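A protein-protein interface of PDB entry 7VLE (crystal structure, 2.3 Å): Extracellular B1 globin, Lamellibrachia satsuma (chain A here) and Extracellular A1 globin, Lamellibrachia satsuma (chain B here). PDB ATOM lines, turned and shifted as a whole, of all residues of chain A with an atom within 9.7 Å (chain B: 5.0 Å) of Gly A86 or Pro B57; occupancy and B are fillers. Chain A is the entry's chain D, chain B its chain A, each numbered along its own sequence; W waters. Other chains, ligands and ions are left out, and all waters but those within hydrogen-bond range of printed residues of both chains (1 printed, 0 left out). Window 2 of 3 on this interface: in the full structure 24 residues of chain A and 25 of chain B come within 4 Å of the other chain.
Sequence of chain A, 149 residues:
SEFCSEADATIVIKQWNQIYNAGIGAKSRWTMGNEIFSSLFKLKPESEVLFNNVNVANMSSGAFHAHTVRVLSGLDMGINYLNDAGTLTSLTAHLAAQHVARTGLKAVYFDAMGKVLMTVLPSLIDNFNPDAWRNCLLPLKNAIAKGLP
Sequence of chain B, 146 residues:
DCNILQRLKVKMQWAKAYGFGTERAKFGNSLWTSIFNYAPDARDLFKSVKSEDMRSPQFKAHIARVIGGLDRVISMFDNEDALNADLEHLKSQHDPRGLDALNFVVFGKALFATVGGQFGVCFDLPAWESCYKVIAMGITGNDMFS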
ATOM      1  N   PHE A   3       8.316   9.253  13.545  1.00  0.00           N
ATOM      2  CA  PHE A   3       7.020   8.797  13.054  1.00  0.00           C
ATOM      3  C   PHE A   3       7.026   8.624  11.536  1.00  0.00           C
ATOM      4  O   PHE A   3       7.155   7.504  11.039  1.00  0.00           O
ATOM      5  CB  PHE A   3       5.918   9.770  13.475  1.00  0.00           C
ATOM      6  CG  PHE A   3       5.238   9.390  14.760  1.00  0.00           C
ATOM      7  CD1 PHE A   3       5.617   9.966  15.962  1.00  0.00           C
ATOM      8  CD2 PHE A   3       4.226   8.446  14.765  1.00  0.00           C
ATOM      9  CE1 PHE A   3       4.991   9.609  17.144  1.00  0.00           C
ATOM     10  CE2 PHE A   3       3.598   8.085  15.940  1.00  0.00           C
ATOM     11  CZ  PHE A   3       3.981   8.667  17.132  1.00  0.00           C
ATOM     12  N   TYR A  81      -0.821  16.350  13.968  1.00  0.00           N
ATOM     13  CA  TYR A  81       0.383  16.541  14.765  1.00  0.00           C
ATOM     14  C   TYR A  81       1.512  15.630  14.298  1.00  0.00           C
ATOM     15  O   TYR A  81       2.428  15.329  15.069  1.00  0.00           O
ATOM     16  CB  TYR A  81       0.081  16.322  16.250  1.00  0.00           C
ATOM     17  CG  TYR A  81      -0.592  17.510  16.906  1.00  0.00           C
ATOM     18  CD1 TYR A  81       0.155  18.461  17.589  1.00  0.00           C
ATOM     19  CD2 TYR A  81      -1.968  17.686  16.833  1.00  0.00           C
ATOM     20  CE1 TYR A  81      -0.450  19.550  18.187  1.00  0.00           C
ATOM     21  CE2 TYR A  81      -2.582  18.774  17.428  1.00  0.00           C
ATOM     22  CZ  TYR A  81      -1.817  19.702  18.105  1.00  0.00           C
ATOM     23  OH  TYR A  81      -2.422  20.786  18.699  1.00  0.00           O
ATOM     24  N   LEU A  82       1.455  15.192  13.036  1.00  0.00           N
ATOM     25  CA  LEU A  82       2.487  14.319  12.487  1.00  0.00           C
ATOM     26  C   LEU A  82       3.848  15.002  12.450  1.00  0.00           C
ATOM     27  O   LEU A  82       4.881  14.331  12.552  1.00  0.00           O
ATOM     28  CB  LEU A  82       2.092  13.862  11.082  1.00  0.00           C
ATOM     29  CG  LEU A  82       1.092  12.711  10.974  1.00  0.00           C
ATOM     30  CD1 LEU A  82       0.651  12.513   9.531  1.00  0.00           C
ATOM     31  CD2 LEU A  82       1.697  11.435  11.535  1.00  0.00           C
ATOM     32  N   ASN A  83       3.871  16.323  12.298  1.00  0.00           N
ATOM     33  CA  ASN A  83       5.115  17.077  12.255  1.00  0.00           C
ATOM     34  C   ASN A  83       5.586  17.524  13.633  1.00  0.00           C
ATOM     35  O   ASN A  83       6.659  18.127  13.739  1.00  0.00           O
ATOM     36  CB  ASN A  83       4.957  18.290  11.334  1.00  0.00           C
ATOM     37  CG  ASN A  83       4.827  17.896   9.873  1.00  0.00           C
ATOM     38  OD1 ASN A  83       5.653  17.151   9.345  1.00  0.00           O
ATOM     39  ND2 ASN A  83       3.780  18.384   9.218  1.00  0.00           N
ATOM     40  N   ASP A  84       4.818  17.243  14.684  1.00  0.00           N
ATOM     41  CA  ASP A  84       5.212  17.528  16.063  1.00  0.00           C
ATOM     42  C   ASP A  84       5.367  16.186  16.776  1.00  0.00           C
ATOM     43  O   ASP A  84       4.491  15.747  17.523  1.00  0.00           O
ATOM     44  CB  ASP A  84       4.185  18.427  16.751  1.00  0.00           C
ATOM     45  CG  ASP A  84       4.707  19.025  18.044  1.00  0.00           C
ATOM     46  OD1 ASP A  84       5.697  18.499  18.596  1.00  0.00           O
ATOM     47  OD2 ASP A  84       4.121  20.023  18.513  1.00  0.00           O
ATOM     48  N   ALA A  85       6.517  15.545  16.549  1.00  0.00           N
ATOM     49  CA  ALA A  85       6.722  14.170  16.997  1.00  0.00           C
ATOM     50  C   ALA A  85       6.672  14.051  18.517  1.00  0.00           C
ATOM     51  O   ALA A  85       6.165  13.058  19.051  1.00  0.00           O
ATOM     52  CB  ALA A  85       8.055  13.644  16.467  1.00  0.00           C
ATOM     53  N   GLY A  86       7.213  15.040  19.231  1.00  0.00           N
ATOM     54  CA  GLY A  86       7.177  14.984  20.683  1.00  0.00           C
ATOM     55  C   GLY A  86       5.763  15.031  21.230  1.00  0.00           C
ATOM     56  O   GLY A  86       5.421  14.297  22.161  1.00  0.00           O
ATOM     57  N   THR A  87       4.921  15.886  20.648  1.00  0.00           N
ATOM     58  CA  THR A  87       3.533  15.984  21.086  1.00  0.00           C
ATOM     59  C   THR A  87       2.725  14.774  20.636  1.00  0.00           C
ATOM     60  O   THR A  87       1.832  14.312  21.357  1.00  0.00           O
ATOM     61  CB  THR A  87       2.906  17.269  20.547  1.00  0.00           C
ATOM     62  OG1 THR A  87       3.736  18.385  20.888  1.00  0.00           O
ATOM     63  CG2 THR A  87       1.517  17.474  21.131  1.00  0.00           C
ATOM     64  N   LEU A  88       3.015  14.256  19.440  1.00  0.00           N
ATOM     65  CA  LEU A  88       2.319  13.068  18.965  1.00  0.00           C
ATOM     66  C   LEU A  88       2.606  11.867  19.854  1.00  0.00           C
ATOM     67  O   LEU A  88       1.726  11.025  20.066  1.00  0.00           O
ATOM     68  CB  LEU A  88       2.715  12.773  17.518  1.00  0.00           C
ATOM     69  CG  LEU A  88       1.920  11.678  16.808  1.00  0.00           C
ATOM     70  CD1 LEU A  88       0.431  11.973  16.889  1.00  0.00           C
ATOM     71  CD2 LEU A  88       2.363  11.541  15.359  1.00  0.00           C
ATOM     72  N   THR A  89       3.827  11.780  20.387  1.00  0.00           N
ATOM     73  CA  THR A  89       4.171  10.713  21.322  1.00  0.00           C
ATOM     74  C   THR A  89       3.289  10.766  22.563  1.00  0.00           C
ATOM     75  O   THR A  89       2.774   9.740  23.021  1.00  0.00           O
ATOM     76  CB  THR A  89       5.645  10.822  21.715  1.00  0.00           C
ATOM     77  OG1 THR A  89       6.467  10.711  20.546  1.00  0.00           O
ATOM     78  CG2 THR A  89       6.017   9.729  22.704  1.00  0.00           C
ATOM     79  N   SER A  90       3.114  11.964  23.126  1.00  0.00           N
ATOM     80  CA  SER A  90       2.253  12.125  24.293  1.00  0.00           C
ATOM     81  C   SER A  90       0.795  11.858  23.943  1.00  0.00           C
ATOM     82  O   SER A  90       0.071  11.218  24.716  1.00  0.00           O
ATOM     83  CB  SER A  90       2.420  13.533  24.867  1.00  0.00           C
ATOM     84  OG  SER A  90       1.546  13.753  25.959  1.00  0.00           O
ATOM     85  N   LEU A  91       0.352  12.338  22.778  1.00  0.00           N
ATOM     86  CA  LEU A  91      -1.028  12.135  22.350  1.00  0.00           C
ATOM     87  C   LEU A  91      -1.339  10.659  22.135  1.00  0.00           C
ATOM     88  O   LEU A  91      -2.434  10.191  22.471  1.00  0.00           O
ATOM     89  CB  LEU A  91      -1.294  12.923  21.068  1.00  0.00           C
ATOM     90  CG  LEU A  91      -1.472  14.435  21.204  1.00  0.00           C
ATOM     91  CD1 LEU A  91      -1.360  15.112  19.848  1.00  0.00           C
ATOM     92  CD2 LEU A  91      -2.814  14.738  21.845  1.00  0.00           C
ATOM     93  N   THR A  92      -0.395   9.913  21.559  1.00  0.00           N
ATOM     94  CA  THR A  92      -0.610   8.487  21.335  1.00  0.00           C
ATOM     95  C   THR A  92      -0.446   7.682  22.616  1.00  0.00           C
ATOM     96  O   THR A  92      -1.106   6.650  22.781  1.00  0.00           O
ATOM     97  CB  THR A  92       0.351   7.961  20.266  1.00  0.00           C
ATOM     98  OG1 THR A  92       1.699   8.305  20.616  1.00  0.00           O
ATOM     99  CG2 THR A  92       0.014   8.550  18.906  1.00  0.00           C
ATOM    100  N   ALA A  93       0.431   8.131  23.519  1.00  0.00           N
ATOM    101  CA  ALA A  93       0.549   7.490  24.823  1.00  0.00           C
ATOM    102  C   ALA A  93      -0.762   7.574  25.592  1.00  0.00           C
ATOM    103  O   ALA A  93      -1.177   6.606  26.240  1.00  0.00           O
ATOM    104  CB  ALA A  93       1.681   8.134  25.621  1.00  0.00           C
ATOM    105  N   HIS A  94      -1.426   8.731  25.529  1.00  0.00           N
ATOM    106  CA  HIS A  94      -2.722   8.893  26.179  1.00  0.00           C
ATOM    107  C   HIS A  94      -3.781   8.010  25.531  1.00  0.00           C
ATOM    108  O   HIS A  94      -4.577   7.370  26.229  1.00  0.00           O
ATOM    109  CB  HIS A  94      -3.140  10.361  26.126  1.00  0.00           C
ATOM    110  CG  HIS A  94      -4.442  10.646  26.806  1.00  0.00           C
ATOM    111  ND1 HIS A  94      -4.527  10.976  28.140  1.00  0.00           N
ATOM    112  CD2 HIS A  94      -5.713  10.650  26.336  1.00  0.00           C
ATOM    113  CE1 HIS A  94      -5.792  11.172  28.464  1.00  0.00           C
ATOM    114  NE2 HIS A  94      -6.533  10.980  27.388  1.00  0.00           N
ATOM    115  N   ARG B  55       4.758  24.738  26.742  1.00  0.00           N
ATOM    116  CA  ARG B  55       5.464  24.290  25.553  1.00  0.00           C
ATOM    117  C   ARG B  55       5.805  22.810  25.613  1.00  0.00           C
ATOM    118  O   ARG B  55       6.222  22.239  24.599  1.00  0.00           O
ATOM    119  CB  ARG B  55       6.739  25.118  25.385  1.00  0.00           C
ATOM    120  CG  ARG B  55       6.665  26.443  26.133  1.00  0.00           C
ATOM    121  CD  ARG B  55       8.039  27.012  26.419  1.00  0.00           C
ATOM    122  NE  ARG B  55       8.530  27.833  25.319  1.00  0.00           N
ATOM    123  CZ  ARG B  55       9.750  28.354  25.268  1.00  0.00           C
ATOM    124  NH1 ARG B  55      10.114  29.093  24.230  1.00  0.00           N
ATOM    125  NH2 ARG B  55      10.608  28.132  26.254  1.00  0.00           N
ATOM    126  N   SER B  56       5.627  22.188  26.776  1.00  0.00           N
ATOM    127  CA  SER B  56       5.909  20.775  26.941  1.00  0.00           C
ATOM    128  C   SER B  56       4.976  19.945  26.063  1.00  0.00           C
ATOM    129  O   SER B  56       3.836  20.342  25.799  1.00  0.00           O
ATOM    130  CB  SER B  56       5.738  20.365  28.403  1.00  0.00           C
ATOM    131  OG  SER B  56       4.365  20.281  28.746  1.00  0.00           O
ATOM    132  N   PRO B  57       5.436  18.782  25.597  1.00  0.00           N
ATOM    133  CA  PRO B  57       4.546  17.893  24.835  1.00  0.00           C
ATOM    134  C   PRO B  57       3.352  17.421  25.640  1.00  0.00           C
ATOM    135  O   PRO B  57       2.334  17.041  25.050  1.00  0.00           O
ATOM    136  CB  PRO B  57       5.465  16.724  24.453  1.00  0.00           C
ATOM    137  CG  PRO B  57       6.548  16.744  25.491  1.00  0.00           C
ATOM    138  CD  PRO B  57       6.767  18.191  25.812  1.00  0.00           C
ATOM    139  N   GLN B  58       3.449  17.442  26.971  1.00  0.00           N
ATOM    140  CA  GLN B  58       2.330  17.044  27.816  1.00  0.00           C
ATOM    141  C   GLN B  58       1.193  18.054  27.736  1.00  0.00           C
ATOM    142  O   GLN B  58       0.033  17.680  27.531  1.00  0.00           O
ATOM    143  CB  GLN B  58       2.798  16.880  29.262  1.00  0.00           C
ATOM    144  CG  GLN B  58       3.590  15.611  29.536  1.00  0.00           C
ATOM    145  CD  GLN B  58       4.956  15.613  28.879  1.00  0.00           C
ATOM    146  OE1 GLN B  58       5.615  16.648  28.786  1.00  0.00           O
ATOM    147  NE2 GLN B  58       5.387  14.446  28.413  1.00  0.00           N
ATOM    148  N   PHE B  59       1.503  19.341  27.904  1.00  0.00           N
ATOM    149  CA  PHE B  59       0.446  20.345  27.858  1.00  0.00           C
ATOM    150  C   PHE B  59      -0.016  20.593  26.430  1.00  0.00           C
ATOM    151  O   PHE B  59      -1.201  20.854  26.192  1.00  0.00           O
ATOM    152  CB  PHE B  59       0.904  21.650  28.501  1.00  0.00           C
ATOM    153  CG  PHE B  59      -0.226  22.600  28.770  1.00  0.00           C
ATOM    154  CD1 PHE B  59      -0.366  23.769  28.040  1.00  0.00           C
ATOM    155  CD2 PHE B  59      -1.173  22.303  29.735  1.00  0.00           C
ATOM    156  CE1 PHE B  59      -1.416  24.633  28.287  1.00  0.00           C
ATOM    157  CE2 PHE B  59      -2.223  23.159  29.985  1.00  0.00           C
ATOM    158  CZ  PHE B  59      -2.346  24.327  29.261  1.00  0.00           C
ATOM    159  N   LYS B  60       0.909  20.534  25.467  1.00  0.00           N
ATOM    160  CA  LYS B  60       0.518  20.597  24.062  1.00  0.00           C
ATOM    161  C   LYS B  60      -0.468  19.489  23.722  1.00  0.00           C
ATOM    162  O   LYS B  60      -1.414  19.699  22.955  1.00  0.00           O
ATOM    163  CB  LYS B  60       1.751  20.499  23.163  1.00  0.00           C
ATOM    164  CG  LYS B  60       2.590  21.760  23.070  1.00  0.00           C
ATOM    165  CD  LYS B  60       3.728  21.552  22.080  1.00  0.00           C
ATOM    166  CE  LYS B  60       4.523  22.824  21.848  1.00  0.00           C
ATOM    167  NZ  LYS B  60       5.608  22.613  20.848  1.00  0.00           N
ATOM    168  N   ALA B  61      -0.258  18.297  24.288  1.00  0.00           N
ATOM    169  CA  ALA B  61      -1.200  17.200  24.091  1.00  0.00           C
ATOM    170  C   ALA B  61      -2.555  17.526  24.702  1.00  0.00           C
ATOM    171  O   ALA B  61      -3.600  17.224  24.113  1.00  0.00           O
ATOM    172  CB  ALA B  61      -0.638  15.914  24.696  1.00  0.00           C
HETATM  173  O   HOH W   1       3.545  12.529  28.036  1.00  0.00           O
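NZ of Lys B60 is in salt-bridge range of OD2 of Asp A84 (3.8 Å).
The side-chain hydroxyl (OG) of Ser B56 lies close to the backbone NH (N) of Gln B58.
The side-chain carboxylate of Asp A84 is in hydrogen-bond range of the side-chain hydroxyl of Thr A87, at 2.9 Å.
O of Gly A86 touches CB of Pro B57, at 3.3 Å.
Thr A87 touches Pro B57.
Thr A87 touches Lys B60.
CG2 of Thr A87 touches N of Ala B61 (3.7 Å).
OG of Ser A90 touches O of Pro B57 (3.5 Å).
CA of Gln B58 touches OG of Ser A90, 3.9 Å away.
Ala B61 touches Ser A90.
Leu A91 touches Ala B61.
Tyr A81 touches none of the printed residues of chain B.
Of the printed residues of chain B, Asp A84 touches Lys B60 (3.8 Å).
Ala A85 touches none of the printed residues of chain B.
Of chain B, only Pro B57 comes within 4 Å of Gly A86.
Of the printed residues of chain B, Ser A90 touches Pro B57, Gln B58 and Ala B61.
Pro B57 touches just these residues of chain A: Gly A86, Thr A87 and Ser A90.
Of the printed residues of chain A, Ala B61 touches Thr A87, Ser A90 and Leu A91.
The nearest printed residue of chain B that does not touch Gly A86 is Gln B58 (6.1 Å).
Hydrophobic or aromatic side chains of chain B that line the printed part of chain A: Pro B57 and Ala B61.
Along chain B the printed residues that touch a printed residue of chain A span positions 57 to 61.
Of the 15 printed residues of chain A, 5 touch a printed residue of chain B.
Among the printed residues, 9 pairs touch across the chains.
Water W1 lies within hydrogen-bond range of NE2 of Gln B58 (2.7 Å) and OG of Ser A90 (3.1 Å).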
